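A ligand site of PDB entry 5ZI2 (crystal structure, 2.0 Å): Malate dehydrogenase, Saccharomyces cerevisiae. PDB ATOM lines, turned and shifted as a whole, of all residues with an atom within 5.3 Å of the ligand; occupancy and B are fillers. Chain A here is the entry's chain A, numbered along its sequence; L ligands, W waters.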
ATOM      1  N   LEU A   9       9.837  23.415  10.733  1.00  0.00           N
ATOM      2  CA  LEU A   9       8.906  23.537  11.886  1.00  0.00           C
ATOM      3  C   LEU A   9       9.063  22.279  12.756  1.00  0.00           C
ATOM      4  O   LEU A   9       8.678  21.181  12.352  1.00  0.00           O
ATOM      5  CB  LEU A   9       7.465  23.769  11.395  1.00  0.00           C
ATOM      6  CG  LEU A   9       7.226  24.715  10.204  1.00  0.00           C
ATOM      7  CD1 LEU A   9       5.746  24.797   9.872  1.00  0.00           C
ATOM      8  CD2 LEU A   9       7.757  26.116  10.469  1.00  0.00           C
ATOM      9  N   GLY A  10       9.591  22.448  13.971  1.00  0.00           N
ATOM     10  CA  GLY A  10       9.995  21.356  14.823  1.00  0.00           C
ATOM     11  C   GLY A  10      11.501  21.105  14.745  1.00  0.00           C
ATOM     12  O   GLY A  10      11.902  19.962  14.887  1.00  0.00           O
ATOM     13  N   SER A  12      14.085  21.704  16.655  1.00  0.00           N
ATOM     14  CA  SER A  12      14.870  21.448  17.871  1.00  0.00           C
ATOM     15  C   SER A  12      14.804  20.046  18.330  1.00  0.00           C
ATOM     16  O   SER A  12      15.453  19.718  19.265  1.00  0.00           O
ATOM     17  CB  SER A  12      14.304  22.317  19.028  1.00  0.00           C
ATOM     18  OG  SER A  12      14.491  23.671  18.680  1.00  0.00           O
ATOM     19  N   GLY A  13      13.995  19.231  17.693  1.00  0.00           N
ATOM     20  CA  GLY A  13      13.828  17.867  18.121  1.00  0.00           C
ATOM     21  C   GLY A  13      14.910  16.918  17.688  1.00  0.00           C
ATOM     22  O   GLY A  13      15.927  17.329  17.037  1.00  0.00           O
ATOM     23  N   GLY A  14      14.631  15.673  17.995  1.00  0.00           N
ATOM     24  CA  GLY A  14      15.447  14.518  17.631  1.00  0.00           C
ATOM     25  C   GLY A  14      15.781  14.406  16.143  1.00  0.00           C
ATOM     26  O   GLY A  14      16.926  14.278  15.772  1.00  0.00           O
ATOM     27  N   VAL A  15      14.754  14.536  15.325  1.00  0.00           N
ATOM     28  CA  VAL A  15      14.896  14.540  13.886  1.00  0.00           C
ATOM     29  C   VAL A  15      15.282  15.948  13.460  1.00  0.00           C
ATOM     30  O   VAL A  15      16.165  16.115  12.658  1.00  0.00           O
ATOM     31  CB  VAL A  15      13.579  14.135  13.216  1.00  0.00           C
ATOM     32  CG1 VAL A  15      13.637  14.317  11.686  1.00  0.00           C
ATOM     33  CG2 VAL A  15      13.194  12.677  13.592  1.00  0.00           C
ATOM     34  N   GLY A  16      14.588  16.954  13.996  1.00  0.00           N
ATOM     35  CA  GLY A  16      14.734  18.348  13.598  1.00  0.00           C
ATOM     36  C   GLY A  16      16.143  18.895  13.639  1.00  0.00           C
ATOM     37  O   GLY A  16      16.587  19.624  12.723  1.00  0.00           O
ATOM     38  N   TYR A  35      12.159  26.929  13.304  1.00  0.00           N
ATOM     39  CA  TYR A  35      11.096  27.258  14.226  1.00  0.00           C
ATOM     40  C   TYR A  35      10.852  26.053  15.143  1.00  0.00           C
ATOM     41  O   TYR A  35      10.838  24.893  14.702  1.00  0.00           O
ATOM     42  CB  TYR A  35       9.795  27.604  13.476  1.00  0.00           C
ATOM     43  CG  TYR A  35       8.643  27.801  14.427  1.00  0.00           C
ATOM     44  CD1 TYR A  35       8.483  29.047  15.107  1.00  0.00           C
ATOM     45  CD2 TYR A  35       7.761  26.763  14.719  1.00  0.00           C
ATOM     46  CE1 TYR A  35       7.423  29.236  15.979  1.00  0.00           C
ATOM     47  CE2 TYR A  35       6.740  26.943  15.612  1.00  0.00           C
ATOM     48  CZ  TYR A  35       6.561  28.199  16.211  1.00  0.00           C
ATOM     49  OH  TYR A  35       5.551  28.339  17.123  1.00  0.00           O
ATOM     50  N   ASP A  36      10.596  26.347  16.401  1.00  0.00           N
ATOM     51  CA  ASP A  36      10.128  25.337  17.317  1.00  0.00           C
ATOM     52  C   ASP A  36       9.465  26.044  18.512  1.00  0.00           C
ATOM     53  O   ASP A  36       9.590  27.277  18.674  1.00  0.00           O
ATOM     54  CB  ASP A  36      11.311  24.500  17.766  1.00  0.00           C
ATOM     55  CG  ASP A  36      10.924  23.132  18.252  1.00  0.00           C
ATOM     56  OD1 ASP A  36      10.336  23.070  19.357  1.00  0.00           O
ATOM     57  OD2 ASP A  36      11.269  22.089  17.614  1.00  0.00           O
ATOM     58  N   ILE A  37       8.773  25.270  19.326  1.00  0.00           N
ATOM     59  CA  ILE A  37       8.243  25.799  20.563  1.00  0.00           C
ATOM     60  C   ILE A  37       9.339  26.140  21.572  1.00  0.00           C
ATOM     61  O   ILE A  37       9.135  27.055  22.331  1.00  0.00           O
ATOM     62  CB  ILE A  37       7.075  24.966  21.153  1.00  0.00           C
ATOM     63  CG1 ILE A  37       7.489  23.563  21.545  1.00  0.00           C
ATOM     64  CG2 ILE A  37       5.871  24.993  20.183  1.00  0.00           C
ATOM     65  CD1 ILE A  37       6.292  22.700  21.955  1.00  0.00           C
ATOM     66  N   ARG A  38      10.513  25.482  21.510  1.00  0.00           N
ATOM     67  CA  ARG A  38      11.699  25.905  22.270  1.00  0.00           C
ATOM     68  C   ARG A  38      12.998  25.771  21.440  1.00  0.00           C
ATOM     69  O   ARG A  38      13.112  24.903  20.540  1.00  0.00           O
ATOM     70  CB  ARG A  38      11.805  25.046  23.530  1.00  0.00           C
ATOM     71  CG  ARG A  38      11.747  23.535  23.219  1.00  0.00           C
ATOM     72  CD  ARG A  38      12.105  22.661  24.411  1.00  0.00           C
ATOM     73  NE  ARG A  38      13.508  22.848  24.822  1.00  0.00           N
ATOM     74  CZ  ARG A  38      14.594  22.269  24.280  1.00  0.00           C
ATOM     75  NH1 ARG A  38      14.508  21.418  23.259  1.00  0.00           N
ATOM     76  NH2 ARG A  38      15.805  22.573  24.760  1.00  0.00           N
ATOM     77  N   PRO A  77       9.158  18.211  10.714  1.00  0.00           N
ATOM     78  CA  PRO A  77       9.513  17.097  11.596  1.00  0.00           C
ATOM     79  C   PRO A  77       8.938  17.285  13.022  1.00  0.00           C
ATOM     80  O   PRO A  77       9.257  16.511  13.854  1.00  0.00           O
ATOM     81  CB  PRO A  77      11.041  17.177  11.658  1.00  0.00           C
ATOM     82  CG  PRO A  77      11.283  18.642  11.591  1.00  0.00           C
ATOM     83  CD  PRO A  77      10.280  19.193  10.633  1.00  0.00           C
ATOM     84  N   ALA A  78       8.126  18.310  13.266  1.00  0.00           N
ATOM     85  CA  ALA A  78       7.413  18.475  14.491  1.00  0.00           C
ATOM     86  C   ALA A  78       6.553  17.278  14.853  1.00  0.00           C
ATOM     87  O   ALA A  78       5.952  16.627  14.018  1.00  0.00           O
ATOM     88  CB  ALA A  78       6.549  19.719  14.425  1.00  0.00           C
ATOM     89  N   GLY A  79       6.479  16.966  16.142  1.00  0.00           N
ATOM     90  CA  GLY A  79       5.638  15.839  16.495  1.00  0.00           C
ATOM     91  C   GLY A  79       6.038  15.306  17.857  1.00  0.00           C
ATOM     92  O   GLY A  79       6.942  15.843  18.545  1.00  0.00           O
ATOM     93  N   VAL A  80       5.376  14.223  18.201  1.00  0.00           N
ATOM     94  CA  VAL A  80       5.732  13.439  19.404  1.00  0.00           C
ATOM     95  C   VAL A  80       6.153  12.077  18.836  1.00  0.00           C
ATOM     96  O   VAL A  80       5.401  11.443  18.080  1.00  0.00           O
ATOM     97  CB  VAL A  80       4.495  13.374  20.364  1.00  0.00           C
ATOM     98  CG1 VAL A  80       4.754  12.428  21.525  1.00  0.00           C
ATOM     99  CG2 VAL A  80       4.194  14.778  20.903  1.00  0.00           C
ATOM    100  N   PRO A  81       7.349  11.620  19.205  1.00  0.00           N
ATOM    101  CA  PRO A  81       7.809  10.289  18.708  1.00  0.00           C
ATOM    102  C   PRO A  81       7.323   9.159  19.613  1.00  0.00           C
ATOM    103  O   PRO A  81       6.840   9.399  20.709  1.00  0.00           O
ATOM    104  CB  PRO A  81       9.306  10.388  18.850  1.00  0.00           C
ATOM    105  CG  PRO A  81       9.490  11.231  20.102  1.00  0.00           C
ATOM    106  CD  PRO A  81       8.340  12.229  20.103  1.00  0.00           C
ATOM    107  N   ARG A  82       7.550   7.943  19.164  1.00  0.00           N
ATOM    108  CA  ARG A  82       7.198   6.736  19.920  1.00  0.00           C
ATOM    109  C   ARG A  82       7.938   6.719  21.216  1.00  0.00           C
ATOM    110  O   ARG A  82       9.090   7.141  21.275  1.00  0.00           O
ATOM    111  CB  ARG A  82       7.578   5.493  19.152  1.00  0.00           C
ATOM    112  CG  ARG A  82       6.701   5.327  17.935  1.00  0.00           C
ATOM    113  CD  ARG A  82       7.219   4.217  17.058  1.00  0.00           C
ATOM    114  NE  ARG A  82       7.129   2.935  17.747  1.00  0.00           N
ATOM    115  CZ  ARG A  82       7.376   1.770  17.168  1.00  0.00           C
ATOM    116  NH1 ARG A  82       7.747   1.708  15.881  1.00  0.00           N
ATOM    117  NH2 ARG A  82       7.282   0.657  17.876  1.00  0.00           N
ATOM    118  N   LYS A  83       7.257   6.345  22.281  1.00  0.00           N
ATOM    119  CA  LYS A  83       7.909   6.237  23.596  1.00  0.00           C
ATOM    120  C   LYS A  83       7.047   5.400  24.528  1.00  0.00           C
ATOM    121  O   LYS A  83       5.818   5.396  24.399  1.00  0.00           O
ATOM    122  CB  LYS A  83       8.257   7.604  24.219  1.00  0.00           C
ATOM    123  CG  LYS A  83       7.117   8.401  24.801  1.00  0.00           C
ATOM    124  CD  LYS A  83       7.447   9.888  24.945  1.00  0.00           C
ATOM    125  CE  LYS A  83       7.504  10.620  23.596  1.00  0.00           C
ATOM    126  NZ  LYS A  83       8.248  11.905  23.662  1.00  0.00           N
ATOM    127  N   ASN A  95       0.091  14.130  17.630  1.00  0.00           N
ATOM    128  CA  ASN A  95       0.562  14.630  16.314  1.00  0.00           C
ATOM    129  C   ASN A  95      -0.433  15.262  15.386  1.00  0.00           C
ATOM    130  O   ASN A  95      -0.115  16.189  14.620  1.00  0.00           O
ATOM    131  CB  ASN A  95       1.309  13.515  15.629  1.00  0.00           C
ATOM    132  CG  ASN A  95       2.608  13.300  16.309  1.00  0.00           C
ATOM    133  OD1 ASN A  95       3.085  14.199  16.983  1.00  0.00           O
ATOM    134  ND2 ASN A  95       3.040  12.118  16.381  1.00  0.00           N
ATOM    135  N   ILE A  98      -0.702  18.877  16.457  1.00  0.00           N
ATOM    136  CA  ILE A  98       0.478  19.590  16.057  1.00  0.00           C
ATOM    137  C   ILE A  98       0.464  19.861  14.527  1.00  0.00           C
ATOM    138  O   ILE A  98       0.616  20.984  14.129  1.00  0.00           O
ATOM    139  CB  ILE A  98       1.740  18.804  16.496  1.00  0.00           C
ATOM    140  CG1 ILE A  98       1.885  18.946  18.028  1.00  0.00           C
ATOM    141  CG2 ILE A  98       2.996  19.299  15.756  1.00  0.00           C
ATOM    142  CD1 ILE A  98       2.731  17.872  18.643  1.00  0.00           C
ATOM    143  N   SER A 101      -2.269  22.499  13.467  1.00  0.00           N
ATOM    144  CA  SER A 101      -1.828  23.827  13.832  1.00  0.00           C
ATOM    145  C   SER A 101      -0.701  24.360  12.921  1.00  0.00           C
ATOM    146  O   SER A 101      -0.710  25.520  12.512  1.00  0.00           O
ATOM    147  CB  SER A 101      -1.258  23.787  15.226  1.00  0.00           C
ATOM    148  OG  SER A 101      -0.754  25.037  15.561  1.00  0.00           O
ATOM    149  N   LEU A 102       0.298  23.519  12.628  1.00  0.00           N
ATOM    150  CA  LEU A 102       1.416  24.001  11.797  1.00  0.00           C
ATOM    151  C   LEU A 102       1.023  24.215  10.364  1.00  0.00           C
ATOM    152  O   LEU A 102       1.439  25.193   9.738  1.00  0.00           O
ATOM    153  CB  LEU A 102       2.643  23.075  11.876  1.00  0.00           C
ATOM    154  CG  LEU A 102       3.233  23.016  13.321  1.00  0.00           C
ATOM    155  CD1 LEU A 102       4.314  21.926  13.409  1.00  0.00           C
ATOM    156  CD2 LEU A 102       3.804  24.347  13.756  1.00  0.00           C
ATOM    157  N   VAL A 117       5.723  16.648   4.966  1.00  0.00           N
ATOM    158  CA  VAL A 117       5.373  16.130   6.272  1.00  0.00           C
ATOM    159  C   VAL A 117       6.273  14.937   6.609  1.00  0.00           C
ATOM    160  O   VAL A 117       6.238  13.926   5.948  1.00  0.00           O
ATOM    161  CB  VAL A 117       3.899  15.751   6.321  1.00  0.00           C
ATOM    162  CG1 VAL A 117       3.538  15.253   7.747  1.00  0.00           C
ATOM    163  CG2 VAL A 117       3.088  16.996   5.985  1.00  0.00           C
ATOM    164  N   ILE A 118       7.062  15.112   7.635  1.00  0.00           N
ATOM    165  CA  ILE A 118       7.898  14.077   8.231  1.00  0.00           C
ATOM    166  C   ILE A 118       7.210  13.443   9.465  1.00  0.00           C
ATOM    167  O   ILE A 118       7.391  12.246   9.726  1.00  0.00           O
ATOM    168  CB  ILE A 118       9.264  14.684   8.562  1.00  0.00           C
ATOM    169  CG1 ILE A 118      10.061  14.850   7.278  1.00  0.00           C
ATOM    170  CG2 ILE A 118      10.075  13.769   9.398  1.00  0.00           C
ATOM    171  CD1 ILE A 118      11.170  15.882   7.338  1.00  0.00           C
ATOM    172  N   SER A 119       6.390  14.207  10.179  1.00  0.00           N
ATOM    173  CA  SER A 119       5.620  13.721  11.343  1.00  0.00           C
ATOM    174  C   SER A 119       4.937  12.398  11.066  1.00  0.00           C
ATOM    175  O   SER A 119       4.349  12.217   9.992  1.00  0.00           O
ATOM    176  CB  SER A 119       4.467  14.719  11.714  1.00  0.00           C
ATOM    177  OG  SER A 119       4.862  16.057  11.579  1.00  0.00           O
ATOM    178  N   ASN A 120       4.987  11.498  12.056  1.00  0.00           N
ATOM    179  CA  ASN A 120       4.281  10.254  11.990  1.00  0.00           C
ATOM    180  C   ASN A 120       3.054  10.230  12.910  1.00  0.00           C
ATOM    181  O   ASN A 120       3.063  10.870  14.011  1.00  0.00           O
ATOM    182  CB  ASN A 120       5.201   9.112  12.366  1.00  0.00           C
ATOM    183  CG  ASN A 120       5.784   8.404  11.160  1.00  0.00           C
ATOM    184  OD1 ASN A 120       5.106   8.211  10.135  1.00  0.00           O
ATOM    185  ND2 ASN A 120       7.012   7.947  11.309  1.00  0.00           N
ATOM    186  N   VAL A 122       2.533   9.232   9.135  1.00  0.00           N
ATOM    187  CA  VAL A 122       2.293   9.778   7.814  1.00  0.00           C
ATOM    188  C   VAL A 122       0.975   9.413   7.193  1.00  0.00           C
ATOM    189  O   VAL A 122       0.292  10.280   6.658  1.00  0.00           O
ATOM    190  CB  VAL A 122       3.457   9.451   6.872  1.00  0.00           C
ATOM    191  CG1 VAL A 122       3.095   9.665   5.400  1.00  0.00           C
ATOM    192  CG2 VAL A 122       4.597  10.353   7.222  1.00  0.00           C
ATOM    193  N   VAL A 147       6.716  12.437   3.570  1.00  0.00           N
ATOM    194  CA  VAL A 147       8.077  11.953   3.411  1.00  0.00           C
ATOM    195  C   VAL A 147       8.171  10.505   3.950  1.00  0.00           C
ATOM    196  O   VAL A 147       8.236  10.235   5.161  1.00  0.00           O
ATOM    197  CB  VAL A 147       9.124  12.873   4.019  1.00  0.00           C
ATOM    198  CG1 VAL A 147      10.576  12.452   3.671  1.00  0.00           C
ATOM    199  CG2 VAL A 147       8.910  14.330   3.559  1.00  0.00           C
ATOM    200  N   LEU A 150      12.462   7.287   4.162  1.00  0.00           N
ATOM    201  CA  LEU A 150      13.244   6.372   4.957  1.00  0.00           C
ATOM    202  C   LEU A 150      13.054   4.938   4.634  1.00  0.00           C
ATOM    203  O   LEU A 150      13.989   4.156   4.781  1.00  0.00           O
ATOM    204  CB  LEU A 150      12.978   6.586   6.425  1.00  0.00           C
ATOM    205  CG  LEU A 150      13.845   5.872   7.421  1.00  0.00           C
ATOM    206  CD1 LEU A 150      15.363   6.081   7.174  1.00  0.00           C
ATOM    207  CD2 LEU A 150      13.404   6.322   8.848  1.00  0.00           C
ATOM    208  N   HIS A 189       3.504   4.122   5.129  1.00  0.00           N
ATOM    209  CA  HIS A 189       4.704   4.365   5.878  1.00  0.00           C
ATOM    210  C   HIS A 189       4.808   3.606   7.209  1.00  0.00           C
ATOM    211  O   HIS A 189       5.768   3.824   7.976  1.00  0.00           O
ATOM    212  CB  HIS A 189       4.803   5.857   6.130  1.00  0.00           C
ATOM    213  CG  HIS A 189       6.182   6.294   6.442  1.00  0.00           C
ATOM    214  ND1 HIS A 189       7.277   5.835   5.740  1.00  0.00           N
ATOM    215  CD2 HIS A 189       6.659   7.143   7.386  1.00  0.00           C
ATOM    216  CE1 HIS A 189       8.373   6.366   6.249  1.00  0.00           C
ATOM    217  NE2 HIS A 189       8.019   7.189   7.217  1.00  0.00           N
ATOM    218  N   SER A 234      12.363   6.287  18.030  1.00  0.00           N
ATOM    219  CA  SER A 234      12.786   5.535  16.883  1.00  0.00           C
ATOM    220  C   SER A 234      13.897   6.308  16.212  1.00  0.00           C
ATOM    221  O   SER A 234      14.710   6.923  16.889  1.00  0.00           O
ATOM    222  CB  SER A 234      11.629   5.284  15.884  1.00  0.00           C
ATOM    223  OG  SER A 234      11.996   4.231  14.966  1.00  0.00           O
ATOM    224  N   ALA A 235      13.990   6.140  14.903  1.00  0.00           N
ATOM    225  CA  ALA A 235      14.975   6.770  14.121  1.00  0.00           C
ATOM    226  C   ALA A 235      14.904   8.289  14.302  1.00  0.00           C
ATOM    227  O   ALA A 235      13.820   8.958  14.334  1.00  0.00           O
ATOM    228  CB  ALA A 235      14.784   6.367  12.659  1.00  0.00           C
ATOM    229  N   THR A 236      16.062   8.811  14.551  1.00  0.00           N
ATOM    230  CA  THR A 236      16.244  10.235  14.544  1.00  0.00           C
ATOM    231  C   THR A 236      17.257  10.545  13.422  1.00  0.00           C
ATOM    232  O   THR A 236      16.911  11.239  12.470  1.00  0.00           O
ATOM    233  CB  THR A 236      16.694  10.723  15.918  1.00  0.00           C
ATOM    234  OG1 THR A 236      17.846   9.975  16.336  1.00  0.00           O
ATOM    235  CG2 THR A 236      15.559  10.550  16.999  1.00  0.00           C
ATOM    236  N   MET A 239      16.361   9.190   9.934  1.00  0.00           N
ATOM    237  CA  MET A 239      15.240   9.948   9.436  1.00  0.00           C
ATOM    238  C   MET A 239      15.626  11.366   8.990  1.00  0.00           C
ATOM    239  O   MET A 239      15.114  11.867   7.956  1.00  0.00           O
ATOM    240  CB  MET A 239      14.100  10.056  10.457  1.00  0.00           C
ATOM    241  CG  MET A 239      12.987  10.925   9.889  1.00  0.00           C
ATOM    242  SD  MET A 239      12.233  10.161   8.422  1.00  0.00           S
ATOM    243  CE  MET A 239      12.150  11.380   7.052  1.00  0.00           C
HETATM  244  P1  LIG L   1      11.233  14.926  19.528  1.00  0.00           P
HETATM  245  O1  LIG L   1      12.688  14.624  19.699  1.00  0.00           O
HETATM  246  O2  LIG L   1      10.224  14.915  20.650  1.00  0.00           O
HETATM  247  O3  LIG L   1      11.153  16.305  18.718  1.00  0.00           O
HETATM  248  C1  LIG L   1       9.914  16.871  18.349  1.00  0.00           C
HETATM  249  C2  LIG L   1      10.006  18.393  18.231  1.00  0.00           C
HETATM  250  O4  LIG L   1       8.740  18.859  17.821  1.00  0.00           O
HETATM  251  C3  LIG L   1      10.283  19.008  19.624  1.00  0.00           C
HETATM  252  O5  LIG L   1      11.408  19.850  19.503  1.00  0.00           O
HETATM  253  C4  LIG L   1       9.035  19.764  20.014  1.00  0.00           C
HETATM  254  O6  LIG L   1       9.305  21.019  20.667  1.00  0.00           O
HETATM  255  C5  LIG L   1       8.511  20.014  18.630  1.00  0.00           C
HETATM  256  N1  LIG L   1       7.112  20.467  18.590  1.00  0.00           N
HETATM  257  C6  LIG L   1       6.027  19.936  19.181  1.00  0.00           C
HETATM  258  N2  LIG L   1       4.925  20.675  18.853  1.00  0.00           N
HETATM  259  C7  LIG L   1       5.312  21.703  18.076  1.00  0.00           C
HETATM  260  C8  LIG L   1       4.664  22.851  17.432  1.00  0.00           C
HETATM  261  N3  LIG L   1       3.350  23.025  17.562  1.00  0.00           N
HETATM  262  N4  LIG L   1       5.444  23.687  16.719  1.00  0.00           N
HETATM  263  C9  LIG L   1       6.779  23.493  16.559  1.00  0.00           C
HETATM  264  N5  LIG L   1       7.425  22.475  17.134  1.00  0.00           N
HETATM  265  C10 LIG L   1       6.756  21.571  17.888  1.00  0.00           C
HETATM  266  O7  LIG L   1      10.652  13.905  18.403  1.00  0.00           O
HETATM  267  P2  LIG L   1      11.473  13.361  17.069  1.00  0.00           P
HETATM  268  O8  LIG L   1      12.137  14.475  16.345  1.00  0.00           O
HETATM  269  O9  LIG L   1      12.116  12.033  17.393  1.00  0.00           O
HETATM  270  O10 LIG L   1      10.249  12.908  16.099  1.00  0.00           O
HETATM  271  C11 LIG L   1       9.503  13.954  15.464  1.00  0.00           C
HETATM  272  C12 LIG L   1       8.452  13.354  14.575  1.00  0.00           C
HETATM  273  O11 LIG L   1       9.113  12.698  13.470  1.00  0.00           O
HETATM  274  C13 LIG L   1       7.536  12.326  15.237  1.00  0.00           C
HETATM  275  O12 LIG L   1       6.228  12.451  14.687  1.00  0.00           O
HETATM  276  C14 LIG L   1       8.066  10.996  14.780  1.00  0.00           C
HETATM  277  O13 LIG L   1       7.044  10.016  14.821  1.00  0.00           O
HETATM  278  C15 LIG L   1       8.469  11.425  13.344  1.00  0.00           C
HETATM  279  N6  LIG L   1       9.314  10.452  12.639  1.00  0.00           N
HETATM  280  C16 LIG L   1       9.008  10.246  11.327  1.00  0.00           C
HETATM  281  C17 LIG L   1       9.751   9.361  10.542  1.00  0.00           C
HETATM  282  C18 LIG L   1       9.417   9.165   9.079  1.00  0.00           C
HETATM  283  O14 LIG L   1       9.801   8.133   8.561  1.00  0.00           O
HETATM  284  N7  LIG L   1       8.794  10.104   8.305  1.00  0.00           N
HETATM  285  C19 LIG L   1      10.821   8.661  11.130  1.00  0.00           C
HETATM  286  C20 LIG L   1      11.126   8.876  12.473  1.00  0.00           C
HETATM  287  C21 LIG L   1      10.352   9.791  13.207  1.00  0.00           C
HETATM  288  O   HOH W   1      13.038  10.520  19.609  1.00  0.00           O
HETATM  289  O   HOH W   2      12.675  20.013  22.023  1.00  0.00           O
HETATM  290  O   HOH W   3       8.720   7.617  16.303  1.00  0.00           O
HETATM  291  O   HOH W   4      10.631   8.761   5.798  1.00  0.00           O
HETATM  292  O   HOH W   5      11.782   9.657  16.158  1.00  0.00           O
HETATM  293  O   HOH W   6       3.051  20.627  20.738  1.00  0.00           O
HETATM  294  O   HOH W   7      12.115  16.995  15.486  1.00  0.00           O
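NE2 of His 189 lies within hydrogen-bond range of O14 of the ligand, at 2.4 Å. An oxygen (O6) of the ligand sits at hydrogen-bond distance from the side-chain carboxylate of Asp 36 (2.6 Å). N of Gly 14 is in hydrogen-bond range of O1 of the ligand (2.8 Å). O8 of the ligand sits at hydrogen-bond distance from N of Val 15 (2.8 Å). The backbone carbonyl oxygen (O) of Ile 118 sits at hydrogen-bond distance from a nitrogen (N7) of the ligand. O12 of the ligand lies within hydrogen-bond range of N of Asn 120 (3.1 Å). The side-chain sulfur of Met 239 lies close to a nitrogen (N7) of the ligand (3.4 Å). An oxygen (O4) of the ligand is in hydrogen-bond range of the backbone NH (N) of Gly 79 (3.4 Å). An oxygen (O5) of the ligand is in hydrogen-bond range of the backbone NH (N) of Gly 13 (3.2 Å). A nitrogen (N7) of the ligand sits at hydrogen-bond distance from the backbone carbonyl oxygen of Val 147.
The side-chain carboxylate (OD2) of Asp 36 sits at hydrogen-bond distance from the backbone NH (N) of Ser 12 (3.0 Å). OD1 of Asp 36 sits close to N of Arg 38. The side-chain amide oxygen (OD1) of Asn 120 sits at hydrogen-bond distance from the backbone NH (N) of Val 122, 2.9 Å away. The backbone carbonyl oxygen (O) of Val 117 is in hydrogen-bond range of the backbone NH (N) of Val 147 (2.8 Å). The side-chain hydroxyl (OG) of Ser 12 lies within hydrogen-bond range of the backbone carbonyl oxygen (O) of Arg 38, at 2.6 Å. OG of Ser 119 is in hydrogen-bond range of O of Ala 78 (2.7 Å). The backbone NH (N) of Ala 78 lies within hydrogen-bond range of the backbone carbonyl oxygen (O) of Leu 9 (3.1 Å). The backbone NH of Val 80 is in hydrogen-bond range of the side-chain amide oxygen of Asn 95, 2.6 Å away.
Gly 10 touches the ligand (CA to N5, 3.6 Å). Ser 12 touches the ligand (C to O5, 3.6 Å). CE2 of Tyr 35 touches C9 of the ligand, at 3.6 Å. CG1 of Ile 37 touches O6 of the ligand, 3.2 Å away. O of Pro 77 touches C11 of the ligand, at 3.0 Å. CA of Ala 78 touches O4 of the ligand, 3.6 Å away. O of Val 80 touches O12 of the ligand (3.6 Å). Pro 81 touches the ligand (CD to O7, 3.3 Å). Asn 95 touches the ligand (ND2 to O12, 3.6 Å). CD1 of Ile 98 touches N2 of the ligand, 3.6 Å away. Leu 102 touches the ligand (CD2 to N4, 3.5 Å). CA of Ser 119 touches O12 of the ligand, 3.6 Å away. O of Ala 235 touches C20 of the ligand, at 3.3 Å. CG2 of Thr 236 touches O9 of the ligand (3.8 Å). The nearest printed residue that does not touch the ligand is Leu 150 (4.04 Å).
Water W7 lies within hydrogen-bond range of O8 of the ligand, N of Gly 16, O of Gly 10 and O of Pro 77. Water W5 lies within hydrogen-bond range of an oxygen (O9) of the ligand and the backbone carbonyl oxygen of Ala 235. Water W2 bridges NH1 of Arg 38 (2.6 Å) and O5 of the ligand (2.8 Å). Water W3 lies within hydrogen-bond range of the backbone NH (N) of Arg 82 (3.1 Å) and an oxygen (O13) of the ligand (3.3 Å).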
